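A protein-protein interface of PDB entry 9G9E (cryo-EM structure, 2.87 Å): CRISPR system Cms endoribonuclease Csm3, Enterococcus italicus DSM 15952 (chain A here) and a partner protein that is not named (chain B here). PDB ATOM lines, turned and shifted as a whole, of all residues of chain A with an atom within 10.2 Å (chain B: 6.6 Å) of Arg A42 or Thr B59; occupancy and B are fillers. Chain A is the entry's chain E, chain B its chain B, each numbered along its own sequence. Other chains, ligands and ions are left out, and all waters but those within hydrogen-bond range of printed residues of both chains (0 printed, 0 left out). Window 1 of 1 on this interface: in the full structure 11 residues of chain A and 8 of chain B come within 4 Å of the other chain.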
ATOM      1  N   PRO A  34     -31.386 -11.343   8.492  1.00  0.00           N
ATOM      2  CA  PRO A  34     -30.538 -10.887   9.598  1.00  0.00           C
ATOM      3  C   PRO A  34     -29.635  -9.737   9.174  1.00  0.00           C
ATOM      4  O   PRO A  34     -29.510  -9.394   7.997  1.00  0.00           O
ATOM      5  CB  PRO A  34     -29.728 -12.133   9.955  1.00  0.00           C
ATOM      6  CG  PRO A  34     -29.640 -12.884   8.672  1.00  0.00           C
ATOM      7  CD  PRO A  34     -30.946 -12.644   7.960  1.00  0.00           C
ATOM      8  N   VAL A  35     -28.995  -9.137  10.173  1.00  0.00           N
ATOM      9  CA  VAL A  35     -28.062  -8.042   9.959  1.00  0.00           C
ATOM     10  C   VAL A  35     -26.645  -8.551  10.187  1.00  0.00           C
ATOM     11  O   VAL A  35     -26.418  -9.608  10.781  1.00  0.00           O
ATOM     12  CB  VAL A  35     -28.361  -6.835  10.873  1.00  0.00           C
ATOM     13  CG1 VAL A  35     -29.709  -6.235  10.530  1.00  0.00           C
ATOM     14  CG2 VAL A  35     -28.314  -7.250  12.334  1.00  0.00           C
ATOM     15  N   VAL A  36     -25.677  -7.777   9.694  1.00  0.00           N
ATOM     16  CA  VAL A  36     -24.275  -8.116   9.897  1.00  0.00           C
ATOM     17  C   VAL A  36     -23.926  -7.952  11.369  1.00  0.00           C
ATOM     18  O   VAL A  36     -24.261  -6.938  11.996  1.00  0.00           O
ATOM     19  CB  VAL A  36     -23.369  -7.247   9.013  1.00  0.00           C
ATOM     20  CG1 VAL A  36     -23.312  -7.800   7.604  1.00  0.00           C
ATOM     21  CG2 VAL A  36     -23.860  -5.812   9.005  1.00  0.00           C
ATOM     22  N   ARG A  37     -23.258  -8.954  11.928  1.00  0.00           N
ATOM     23  CA  ARG A  37     -22.802  -8.916  13.306  1.00  0.00           C
ATOM     24  C   ARG A  37     -21.327  -9.274  13.357  1.00  0.00           C
ATOM     25  O   ARG A  37     -20.836 -10.068  12.549  1.00  0.00           O
ATOM     26  CB  ARG A  37     -23.599  -9.880  14.198  1.00  0.00           C
ATOM     27  CG  ARG A  37     -25.105  -9.797  14.032  1.00  0.00           C
ATOM     28  CD  ARG A  37     -25.811 -10.738  14.992  1.00  0.00           C
ATOM     29  NE  ARG A  37     -26.075 -10.109  16.280  1.00  0.00           N
ATOM     30  CZ  ARG A  37     -27.211  -9.503  16.599  1.00  0.00           C
ATOM     31  NH1 ARG A  37     -28.214  -9.421  15.742  1.00  0.00           N
ATOM     32  NH2 ARG A  37     -27.342  -8.965  17.809  1.00  0.00           N
ATOM     33  N   ASP A  38     -20.626  -8.681  14.308  1.00  0.00           N
ATOM     34  CA  ASP A  38     -19.247  -9.066  14.559  1.00  0.00           C
ATOM     35  C   ASP A  38     -19.243 -10.461  15.166  1.00  0.00           C
ATOM     36  O   ASP A  38     -19.893 -10.676  16.195  1.00  0.00           O
ATOM     37  CB  ASP A  38     -18.575  -8.066  15.494  1.00  0.00           C
ATOM     38  CG  ASP A  38     -17.127  -8.409  15.770  1.00  0.00           C
ATOM     39  OD1 ASP A  38     -16.401  -8.745  14.811  1.00  0.00           O
ATOM     40  OD2 ASP A  38     -16.714  -8.341  16.946  1.00  0.00           O
ATOM     41  N   PRO A  39     -18.560 -11.437  14.563  1.00  0.00           N
ATOM     42  CA  PRO A  39     -18.606 -12.802  15.114  1.00  0.00           C
ATOM     43  C   PRO A  39     -18.089 -12.903  16.538  1.00  0.00           C
ATOM     44  O   PRO A  39     -18.555 -13.764  17.295  1.00  0.00           O
ATOM     45  CB  PRO A  39     -17.731 -13.599  14.136  1.00  0.00           C
ATOM     46  CG  PRO A  39     -17.763 -12.809  12.870  1.00  0.00           C
ATOM     47  CD  PRO A  39     -17.813 -11.375  13.297  1.00  0.00           C
ATOM     48  N   TYR A  40     -17.139 -12.051  16.927  1.00  0.00           N
ATOM     49  CA  TYR A  40     -16.539 -12.163  18.252  1.00  0.00           C
ATOM     50  C   TYR A  40     -17.523 -11.768  19.349  1.00  0.00           C
ATOM     51  O   TYR A  40     -17.676 -12.486  20.344  1.00  0.00           O
ATOM     52  CB  TYR A  40     -15.275 -11.308  18.325  1.00  0.00           C
ATOM     53  CG  TYR A  40     -14.434 -11.570  19.552  1.00  0.00           C
ATOM     54  CD1 TYR A  40     -13.903 -12.830  19.796  1.00  0.00           C
ATOM     55  CD2 TYR A  40     -14.164 -10.558  20.462  1.00  0.00           C
ATOM     56  CE1 TYR A  40     -13.131 -13.075  20.914  1.00  0.00           C
ATOM     57  CE2 TYR A  40     -13.393 -10.794  21.584  1.00  0.00           C
ATOM     58  CZ  TYR A  40     -12.879 -12.054  21.804  1.00  0.00           C
ATOM     59  OH  TYR A  40     -12.109 -12.293  22.919  1.00  0.00           O
ATOM     60  N   SER A  41     -18.199 -10.631  19.187  1.00  0.00           N
ATOM     61  CA  SER A  41     -19.082 -10.106  20.219  1.00  0.00           C
ATOM     62  C   SER A  41     -20.560 -10.343  19.938  1.00  0.00           C
ATOM     63  O   SER A  41     -21.386 -10.095  20.822  1.00  0.00           O
ATOM     64  CB  SER A  41     -18.839  -8.603  20.407  1.00  0.00           C
ATOM     65  OG  SER A  41     -18.967  -7.909  19.179  1.00  0.00           O
ATOM     66  N   ARG A  42     -20.908 -10.808  18.738  1.00  0.00           N
ATOM     67  CA  ARG A  42     -22.297 -11.025  18.328  1.00  0.00           C
ATOM     68  C   ARG A  42     -23.134  -9.756  18.460  1.00  0.00           C
ATOM     69  O   ARG A  42     -24.321  -9.813  18.789  1.00  0.00           O
ATOM     70  CB  ARG A  42     -22.940 -12.176  19.106  1.00  0.00           C
ATOM     71  CG  ARG A  42     -22.331 -13.536  18.808  1.00  0.00           C
ATOM     72  CD  ARG A  42     -22.938 -14.618  19.683  1.00  0.00           C
ATOM     73  NE  ARG A  42     -24.372 -14.758  19.456  1.00  0.00           N
ATOM     74  CZ  ARG A  42     -24.918 -15.655  18.649  1.00  0.00           C
ATOM     75  NH1 ARG A  42     -24.178 -16.517  17.970  1.00  0.00           N
ATOM     76  NH2 ARG A  42     -26.242 -15.690  18.518  1.00  0.00           N
ATOM     77  N   LEU A  43     -22.517  -8.593  18.203  1.00  0.00           N
ATOM     78  CA  LEU A  43     -23.194  -7.309  18.197  1.00  0.00           C
ATOM     79  C   LEU A  43     -23.340  -6.795  16.770  1.00  0.00           C
ATOM     80  O   LEU A  43     -22.479  -7.051  15.923  1.00  0.00           O
ATOM     81  CB  LEU A  43     -22.419  -6.280  19.026  1.00  0.00           C
ATOM     82  CG  LEU A  43     -22.189  -6.597  20.505  1.00  0.00           C
ATOM     83  CD1 LEU A  43     -21.766  -5.347  21.256  1.00  0.00           C
ATOM     84  CD2 LEU A  43     -23.435  -7.202  21.127  1.00  0.00           C
ATOM     85  N   PRO A  44     -24.418  -6.071  16.470  1.00  0.00           N
ATOM     86  CA  PRO A  44     -24.581  -5.524  15.119  1.00  0.00           C
ATOM     87  C   PRO A  44     -23.449  -4.570  14.770  1.00  0.00           C
ATOM     88  O   PRO A  44     -22.910  -3.866  15.627  1.00  0.00           O
ATOM     89  CB  PRO A  44     -25.931  -4.797  15.184  1.00  0.00           C
ATOM     90  CG  PRO A  44     -26.215  -4.622  16.639  1.00  0.00           C
ATOM     91  CD  PRO A  44     -25.580  -5.785  17.326  1.00  0.00           C
ATOM     92  N   ILE A  45     -23.087  -4.557  13.488  1.00  0.00           N
ATOM     93  CA  ILE A  45     -21.935  -3.812  13.005  1.00  0.00           C
ATOM     94  C   ILE A  45     -22.333  -3.035  11.758  1.00  0.00           C
ATOM     95  O   ILE A  45     -23.289  -3.377  11.058  1.00  0.00           O
ATOM     96  CB  ILE A  45     -20.735  -4.743  12.709  1.00  0.00           C
ATOM     97  CG1 ILE A  45     -19.423  -3.957  12.676  1.00  0.00           C
ATOM     98  CG2 ILE A  45     -20.945  -5.497  11.404  1.00  0.00           C
ATOM     99  CD1 ILE A  45     -18.253  -4.764  12.171  1.00  0.00           C
ATOM    100  N   PHE A 102     -18.188  -0.265  15.058  1.00  0.00           N
ATOM    101  CA  PHE A 102     -18.595  -1.282  16.014  1.00  0.00           C
ATOM    102  C   PHE A 102     -19.595  -0.711  17.010  1.00  0.00           C
ATOM    103  O   PHE A 102     -19.577   0.482  17.322  1.00  0.00           O
ATOM    104  CB  PHE A 102     -17.380  -1.837  16.758  1.00  0.00           C
ATOM    105  CG  PHE A 102     -16.341  -2.439  15.857  1.00  0.00           C
ATOM    106  CD1 PHE A 102     -16.555  -3.668  15.255  1.00  0.00           C
ATOM    107  CD2 PHE A 102     -15.152  -1.775  15.610  1.00  0.00           C
ATOM    108  CE1 PHE A 102     -15.600  -4.223  14.426  1.00  0.00           C
ATOM    109  CE2 PHE A 102     -14.194  -2.325  14.781  1.00  0.00           C
ATOM    110  CZ  PHE A 102     -14.420  -3.551  14.188  1.00  0.00           C
ATOM    111  N   PHE A 103     -20.482  -1.578  17.492  1.00  0.00           N
ATOM    112  CA  PHE A 103     -21.447  -1.193  18.514  1.00  0.00           C
ATOM    113  C   PHE A 103     -20.731  -0.628  19.732  1.00  0.00           C
ATOM    114  O   PHE A 103     -19.949  -1.326  20.384  1.00  0.00           O
ATOM    115  CB  PHE A 103     -22.296  -2.404  18.904  1.00  0.00           C
ATOM    116  CG  PHE A 103     -23.672  -2.051  19.390  1.00  0.00           C
ATOM    117  CD1 PHE A 103     -23.886  -1.695  20.710  1.00  0.00           C
ATOM    118  CD2 PHE A 103     -24.750  -2.079  18.524  1.00  0.00           C
ATOM    119  CE1 PHE A 103     -25.152  -1.373  21.156  1.00  0.00           C
ATOM    120  CE2 PHE A 103     -26.018  -1.760  18.965  1.00  0.00           C
ATOM    121  CZ  PHE A 103     -26.219  -1.405  20.283  1.00  0.00           C
ATOM    122  N   GLN A 108     -24.121   0.009  24.510  1.00  0.00           N
ATOM    123  CA  GLN A 108     -24.341  -1.295  25.126  1.00  0.00           C
ATOM    124  C   GLN A 108     -24.770  -1.154  26.582  1.00  0.00           C
ATOM    125  O   GLN A 108     -25.683  -1.851  27.037  1.00  0.00           O
ATOM    126  CB  GLN A 108     -23.074  -2.143  25.016  1.00  0.00           C
ATOM    127  CG  GLN A 108     -23.264  -3.597  25.403  1.00  0.00           C
ATOM    128  CD  GLN A 108     -22.066  -4.453  25.044  1.00  0.00           C
ATOM    129  OE1 GLN A 108     -21.151  -4.002  24.357  1.00  0.00           O
ATOM    130  NE2 GLN A 108     -22.065  -5.695  25.512  1.00  0.00           N
ATOM    131  N   ASP A 112     -28.363  -2.260  28.070  1.00  0.00           N
ATOM    132  CA  ASP A 112     -28.467  -3.212  29.171  1.00  0.00           C
ATOM    133  C   ASP A 112     -29.472  -2.731  30.208  1.00  0.00           C
ATOM    134  O   ASP A 112     -30.292  -3.513  30.701  1.00  0.00           O
ATOM    135  CB  ASP A 112     -27.096  -3.437  29.808  1.00  0.00           C
ATOM    136  CG  ASP A 112     -26.170  -4.238  28.919  1.00  0.00           C
ATOM    137  OD1 ASP A 112     -26.575  -4.566  27.786  1.00  0.00           O
ATOM    138  OD2 ASP A 112     -25.038  -4.542  29.352  1.00  0.00           O
ATOM    139  N   LEU A 116     -32.866  -3.926  26.494  1.00  0.00           N
ATOM    140  CA  LEU A 116     -32.999  -3.999  25.048  1.00  0.00           C
ATOM    141  C   LEU A 116     -32.035  -5.044  24.493  1.00  0.00           C
ATOM    142  O   LEU A 116     -31.006  -5.356  25.095  1.00  0.00           O
ATOM    143  CB  LEU A 116     -32.737  -2.636  24.403  1.00  0.00           C
ATOM    144  CG  LEU A 116     -33.906  -1.649  24.415  1.00  0.00           C
ATOM    145  CD1 LEU A 116     -33.462  -0.282  23.922  1.00  0.00           C
ATOM    146  CD2 LEU A 116     -35.059  -2.176  23.578  1.00  0.00           C
ATOM    147  N   ALA A 117     -32.384  -5.582  23.327  1.00  0.00           N
ATOM    148  CA  ALA A 117     -31.671  -6.710  22.743  1.00  0.00           C
ATOM    149  C   ALA A 117     -30.692  -6.304  21.647  1.00  0.00           C
ATOM    150  O   ALA A 117     -30.243  -7.174  20.893  1.00  0.00           O
ATOM    151  CB  ALA A 117     -32.668  -7.730  22.190  1.00  0.00           C
ATOM    152  N   TYR A 118     -30.388  -5.007  21.522  1.00  0.00           N
ATOM    153  CA  TYR A 118     -29.465  -4.462  20.527  1.00  0.00           C
ATOM    154  C   TYR A 118     -30.059  -4.528  19.126  1.00  0.00           C
ATOM    155  O   TYR A 118     -29.465  -4.019  18.170  1.00  0.00           O
ATOM    156  CB  TYR A 118     -28.117  -5.193  20.528  1.00  0.00           C
ATOM    157  CG  TYR A 118     -27.457  -5.348  21.875  1.00  0.00           C
ATOM    158  CD1 TYR A 118     -27.513  -4.339  22.827  1.00  0.00           C
ATOM    159  CD2 TYR A 118     -26.768  -6.509  22.191  1.00  0.00           C
ATOM    160  CE1 TYR A 118     -26.902  -4.490  24.058  1.00  0.00           C
ATOM    161  CE2 TYR A 118     -26.157  -6.667  23.414  1.00  0.00           C
ATOM    162  CZ  TYR A 118     -26.226  -5.658  24.344  1.00  0.00           C
ATOM    163  OH  TYR A 118     -25.611  -5.826  25.561  1.00  0.00           O
ATOM    164  N   THR A 119     -31.227  -5.150  18.993  1.00  0.00           N
ATOM    165  CA  THR A 119     -31.786  -5.433  17.681  1.00  0.00           C
ATOM    166  C   THR A 119     -33.285  -5.646  17.823  1.00  0.00           C
ATOM    167  O   THR A 119     -33.800  -5.871  18.921  1.00  0.00           O
ATOM    168  CB  THR A 119     -31.118  -6.658  17.045  1.00  0.00           C
ATOM    169  OG1 THR A 119     -31.445  -6.718  15.653  1.00  0.00           O
ATOM    170  CG2 THR A 119     -31.584  -7.937  17.726  1.00  0.00           C
ATOM    171  N   GLU A 140     -34.645  -7.853  10.148  1.00  0.00           N
ATOM    172  CA  GLU A 140     -33.960  -7.472  11.373  1.00  0.00           C
ATOM    173  C   GLU A 140     -33.371  -6.076  11.225  1.00  0.00           C
ATOM    174  O   GLU A 140     -32.839  -5.718  10.172  1.00  0.00           O
ATOM    175  CB  GLU A 140     -32.867  -8.482  11.713  1.00  0.00           C
ATOM    176  CG  GLU A 140     -32.363  -8.377  13.138  1.00  0.00           C
ATOM    177  CD  GLU A 140     -31.449  -9.523  13.523  1.00  0.00           C
ATOM    178  OE1 GLU A 140     -31.267 -10.443  12.700  1.00  0.00           O
ATOM    179  OE2 GLU A 140     -30.918  -9.506  14.652  1.00  0.00           O
ATOM    180  N   VAL A 142     -31.430  -2.610  13.580  1.00  0.00           N
ATOM    181  CA  VAL A 142     -30.743  -2.143  14.777  1.00  0.00           C
ATOM    182  C   VAL A 142     -31.614  -1.083  15.436  1.00  0.00           C
ATOM    183  O   VAL A 142     -32.142  -0.193  14.760  1.00  0.00           O
ATOM    184  CB  VAL A 142     -29.352  -1.589  14.431  1.00  0.00           C
ATOM    185  CG1 VAL A 142     -28.652  -1.093  15.682  1.00  0.00           C
ATOM    186  CG2 VAL A 142     -28.516  -2.653  13.741  1.00  0.00           C
ATOM    187  N   PHE A 148     -22.757   3.755  17.076  1.00  0.00           N
ATOM    188  CA  PHE A 148     -21.597   3.029  16.578  1.00  0.00           C
ATOM    189  C   PHE A 148     -20.367   3.924  16.599  1.00  0.00           C
ATOM    190  O   PHE A 148     -20.455   5.122  16.317  1.00  0.00           O
ATOM    191  CB  PHE A 148     -21.841   2.508  15.157  1.00  0.00           C
ATOM    192  CG  PHE A 148     -22.951   1.500  15.060  1.00  0.00           C
ATOM    193  CD1 PHE A 148     -24.276   1.903  15.022  1.00  0.00           C
ATOM    194  CD2 PHE A 148     -22.668   0.146  15.004  1.00  0.00           C
ATOM    195  CE1 PHE A 148     -25.294   0.976  14.932  1.00  0.00           C
ATOM    196  CE2 PHE A 148     -23.683  -0.786  14.915  1.00  0.00           C
ATOM    197  CZ  PHE A 148     -24.997  -0.370  14.878  1.00  0.00           C
ATOM    198  N   ILE B  54     -34.732 -16.979  24.101  1.00  0.00           N
ATOM    199  CA  ILE B  54     -33.586 -17.856  24.307  1.00  0.00           C
ATOM    200  C   ILE B  54     -32.330 -17.250  23.700  1.00  0.00           C
ATOM    201  O   ILE B  54     -31.268 -17.247  24.328  1.00  0.00           O
ATOM    202  CB  ILE B  54     -33.879 -19.258  23.737  1.00  0.00           C
ATOM    203  CG1 ILE B  54     -34.706 -20.073  24.735  1.00  0.00           C
ATOM    204  CG2 ILE B  54     -32.584 -19.983  23.394  1.00  0.00           C
ATOM    205  CD1 ILE B  54     -34.753 -21.555  24.434  1.00  0.00           C
ATOM    206  N   ASN B  55     -32.427 -16.708  22.481  1.00  0.00           N
ATOM    207  CA  ASN B  55     -31.228 -16.151  21.865  1.00  0.00           C
ATOM    208  C   ASN B  55     -30.821 -14.833  22.516  1.00  0.00           C
ATOM    209  O   ASN B  55     -29.631 -14.510  22.545  1.00  0.00           O
ATOM    210  CB  ASN B  55     -31.400 -15.990  20.346  1.00  0.00           C
ATOM    211  CG  ASN B  55     -32.492 -15.005  19.956  1.00  0.00           C
ATOM    212  OD1 ASN B  55     -32.515 -13.859  20.404  1.00  0.00           O
ATOM    213  ND2 ASN B  55     -33.376 -15.438  19.067  1.00  0.00           N
ATOM    214  N   HIS B  56     -31.774 -14.080  23.071  1.00  0.00           N
ATOM    215  CA  HIS B  56     -31.416 -12.877  23.817  1.00  0.00           C
ATOM    216  C   HIS B  56     -30.628 -13.232  25.072  1.00  0.00           C
ATOM    217  O   HIS B  56     -29.573 -12.644  25.350  1.00  0.00           O
ATOM    218  CB  HIS B  56     -32.681 -12.092  24.172  1.00  0.00           C
ATOM    219  CG  HIS B  56     -32.414 -10.764  24.812  1.00  0.00           C
ATOM    220  ND1 HIS B  56     -33.423  -9.955  25.289  1.00  0.00           N
ATOM    221  CD2 HIS B  56     -31.258 -10.100  25.047  1.00  0.00           C
ATOM    222  CE1 HIS B  56     -32.900  -8.853  25.795  1.00  0.00           C
ATOM    223  NE2 HIS B  56     -31.587  -8.916  25.661  1.00  0.00           N
ATOM    224  N   VAL B  57     -31.122 -14.207  25.839  1.00  0.00           N
ATOM    225  CA  VAL B  57     -30.401 -14.632  27.035  1.00  0.00           C
ATOM    226  C   VAL B  57     -29.059 -15.247  26.648  1.00  0.00           C
ATOM    227  O   VAL B  57     -28.046 -15.061  27.337  1.00  0.00           O
ATOM    228  CB  VAL B  57     -31.270 -15.600  27.861  1.00  0.00           C
ATOM    229  CG1 VAL B  57     -30.413 -16.559  28.665  1.00  0.00           C
ATOM    230  CG2 VAL B  57     -32.206 -14.823  28.773  1.00  0.00           C
ATOM    231  N   TYR B  58     -29.025 -15.963  25.520  1.00  0.00           N
ATOM    232  CA  TYR B  58     -27.787 -16.561  25.039  1.00  0.00           C
ATOM    233  C   TYR B  58     -26.754 -15.500  24.689  1.00  0.00           C
ATOM    234  O   TYR B  58     -25.574 -15.646  25.018  1.00  0.00           O
ATOM    235  CB  TYR B  58     -28.079 -17.453  23.831  1.00  0.00           C
ATOM    236  CG  TYR B  58     -26.850 -17.935  23.094  1.00  0.00           C
ATOM    237  CD1 TYR B  58     -26.150 -19.052  23.531  1.00  0.00           C
ATOM    238  CD2 TYR B  58     -26.401 -17.286  21.952  1.00  0.00           C
ATOM    239  CE1 TYR B  58     -25.030 -19.500  22.856  1.00  0.00           C
ATOM    240  CE2 TYR B  58     -25.283 -17.726  21.274  1.00  0.00           C
ATOM    241  CZ  TYR B  58     -24.601 -18.833  21.729  1.00  0.00           C
ATOM    242  OH  TYR B  58     -23.486 -19.276  21.055  1.00  0.00           O
ATOM    243  N   THR B  59     -27.173 -14.424  24.018  1.00  0.00           N
ATOM    244  CA  THR B  59     -26.231 -13.363  23.678  1.00  0.00           C
ATOM    245  C   THR B  59     -25.766 -12.620  24.923  1.00  0.00           C
ATOM    246  O   THR B  59     -24.598 -12.221  25.014  1.00  0.00           O
ATOM    247  CB  THR B  59     -26.854 -12.388  22.677  1.00  0.00           C
ATOM    248  OG1 THR B  59     -28.237 -12.188  22.992  1.00  0.00           O
ATOM    249  CG2 THR B  59     -26.736 -12.933  21.262  1.00  0.00           C
ATOM    250  N   LYS B  60     -26.663 -12.423  25.894  1.00  0.00           N
ATOM    251  CA  LYS B  60     -26.253 -11.784  27.141  1.00  0.00           C
ATOM    252  C   LYS B  60     -25.222 -12.628  27.883  1.00  0.00           C
ATOM    253  O   LYS B  60     -24.263 -12.091  28.450  1.00  0.00           O
ATOM    254  CB  LYS B  60     -27.470 -11.510  28.024  1.00  0.00           C
ATOM    255  CG  LYS B  60     -27.978 -10.081  27.924  1.00  0.00           C
ATOM    256  CD  LYS B  60     -29.211  -9.865  28.780  1.00  0.00           C
ATOM    257  CE  LYS B  60     -29.517  -8.387  28.948  1.00  0.00           C
ATOM    258  NZ  LYS B  60     -29.648  -7.690  27.639  1.00  0.00           N
ATOM    259  N   VAL B  61     -25.402 -13.950  27.892  1.00  0.00           N
ATOM    260  CA  VAL B  61     -24.407 -14.831  28.497  1.00  0.00           C
ATOM    261  C   VAL B  61     -23.115 -14.814  27.687  1.00  0.00           C
ATOM    262  O   VAL B  61     -22.011 -14.824  28.246  1.00  0.00           O
ATOM    263  CB  VAL B  61     -24.975 -16.255  28.634  1.00  0.00           C
ATOM    264  CG1 VAL B  61     -23.860 -17.268  28.852  1.00  0.00           C
ATOM    265  CG2 VAL B  61     -25.980 -16.316  29.770  1.00  0.00           C
ATOM    266  N   TYR B  62     -23.235 -14.777  26.359  1.00  0.00           N
ATOM    267  CA  TYR B  62     -22.071 -14.801  25.481  1.00  0.00           C
ATOM    268  C   TYR B  62     -21.194 -13.573  25.690  1.00  0.00           C
ATOM    269  O   TYR B  62     -19.961 -13.676  25.695  1.00  0.00           O
ATOM    270  CB  TYR B  62     -22.540 -14.893  24.028  1.00  0.00           C
ATOM    271  CG  TYR B  62     -21.466 -15.221  23.018  1.00  0.00           C
ATOM    272  CD1 TYR B  62     -20.694 -14.220  22.446  1.00  0.00           C
ATOM    273  CD2 TYR B  62     -21.241 -16.531  22.619  1.00  0.00           C
ATOM    274  CE1 TYR B  62     -19.720 -14.516  21.516  1.00  0.00           C
ATOM    275  CE2 TYR B  62     -20.269 -16.836  21.688  1.00  0.00           C
ATOM    276  CZ  TYR B  62     -19.510 -15.825  21.140  1.00  0.00           C
ATOM    277  OH  TYR B  62     -18.539 -16.123  20.214  1.00  0.00           O
ATOM    278  N   ASN B  63     -21.812 -12.401  25.856  1.00  0.00           N
ATOM    279  CA  ASN B  63     -21.038 -11.183  26.078  1.00  0.00           C
ATOM    280  C   ASN B  63     -20.231 -11.267  27.367  1.00  0.00           C
ATOM    281  O   ASN B  63     -19.059 -10.872  27.402  1.00  0.00           O
ATOM    282  CB  ASN B  63     -21.967  -9.969  26.104  1.00  0.00           C
ATOM    283  CG  ASN B  63     -22.230  -9.409  24.722  1.00  0.00           C
ATOM    284  OD1 ASN B  63     -22.897  -8.387  24.570  1.00  0.00           O
ATOM    285  ND2 ASN B  63     -21.706 -10.079  23.703  1.00  0.00           N
ATOM    286  N   SER B  64     -20.836 -11.779  28.435  1.00  0.00           N
ATOM    287  CA  SER B  64     -20.119 -11.953  29.688  1.00  0.00           C
ATOM    288  C   SER B  64     -19.126 -13.104  29.579  1.00  0.00           C
ATOM    289  O   SER B  64     -19.322 -14.058  28.822  1.00  0.00           O
ATOM    290  CB  SER B  64     -21.096 -12.211  30.834  1.00  0.00           C
ATOM    291  OG  SER B  64     -21.504 -13.568  30.861  1.00  0.00           O
ATOM    292  N   PHE B 119     -25.473 -24.181  30.109  1.00  0.00           N
ATOM    293  CA  PHE B 119     -26.395 -23.298  29.403  1.00  0.00           C
ATOM    294  C   PHE B 119     -26.141 -23.316  27.900  1.00  0.00           C
ATOM    295  O   PHE B 119     -27.086 -23.333  27.102  1.00  0.00           O
ATOM    296  CB  PHE B 119     -26.282 -21.875  29.944  1.00  0.00           C
ATOM    297  CG  PHE B 119     -26.990 -20.858  29.104  1.00  0.00           C
ATOM    298  CD1 PHE B 119     -28.373 -20.811  29.071  1.00  0.00           C
ATOM    299  CD2 PHE B 119     -26.274 -19.957  28.334  1.00  0.00           C
ATOM    300  CE1 PHE B 119     -29.027 -19.879  28.293  1.00  0.00           C
ATOM    301  CE2 PHE B 119     -26.923 -19.025  27.555  1.00  0.00           C
ATOM    302  CZ  PHE B 119     -28.300 -18.987  27.534  1.00  0.00           C
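Hydrophobic or aromatic side chains of chain B that line the printed part of chain A: His B56, Tyr B58 and Tyr B62.
Among the printed residues, no Asp or Glu carboxylate lies within 4 Å of a Lys or Arg side-chain nitrogen of the other chain.
Arg A42 touches just these residues of chain B: Tyr B58 (3.4 Å), Thr B59 (3.5 Å) and Tyr B62 (3.6 Å).
Thr B59 touches just one residue of chain A: Arg A42.
Tyr B58 touches just one residue of chain A: Arg A42 (3.4 Å).
Of the printed residues of chain A, His B56 touches Leu A116 and Ala A117.
Of the printed residues of chain B, Leu A43 touches Asn B63.
Printed residues of chain B within 4 Å of Pro A39: Tyr B62 (3.8 Å).
Phe A102 touches none of the printed residues of chain B.
Val B61 touches none of the printed residues of chain A.
The nearest residue of chain A that does not touch Thr B59 is Arg A37 (5.3 Å).
The nearest printed residue of chain B that does not touch Pro A39 is Asn B63 (8.0 Å).
Pro A39 touches Tyr B62 (O to OH, 3.8 Å).
Tyr B62 touches Tyr A40 (CE1 to O, 3.1 Å).
CE2 of Tyr B58 touches CZ of Arg A42, at 3.4 Å.
Arg A42 touches Thr B59.
Arg A42 touches Tyr B62.
Asn B63 touches Leu A43 (OD1 to CD2, 3.7 Å).
Leu A116 touches His B56 (O to NE2, 3.7 Å).
Leu A116 touches Lys B60 (O to NZ, 3.7 Å).
His B56 touches Ala A117 (NE2 to CA, 3.7 Å).
Tyr A118 touches Asn B63 (OH to OD1, 3.9 Å).
The side-chain hydroxyl (OG1) of Thr B59 lies within hydrogen-bond range of the backbone carbonyl oxygen (O) of Asn B55 (2.7 Å).
The side-chain amino group (NZ) of Lys B60 lies within hydrogen-bond range of a ring nitrogen (NE2) of His B56, at 3.0 Å.
The side-chain carboxylate (OD2) of Asp A38 sits at hydrogen-bond distance from the side-chain hydroxyl (OG) of Ser A41, 3.2 Å away.
OD1 of Asp A112 sits at hydrogen-bond distance from OH of Tyr A118.
The side-chain hydroxyl of Thr B59 sits at hydrogen-bond distance from the backbone carbonyl oxygen of His B56 (2.7 Å).
NE of Arg A37 lies within hydrogen-bond range of O of Arg A42, at 3.1 Å.
The side-chain amide oxygen of Asn B63 is in hydrogen-bond range of the side-chain amide nitrogen of Gln A108 (3.0 Å).
O of Ser A41 sits at hydrogen-bond distance from ND2 of Asn B63 (2.9 Å).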
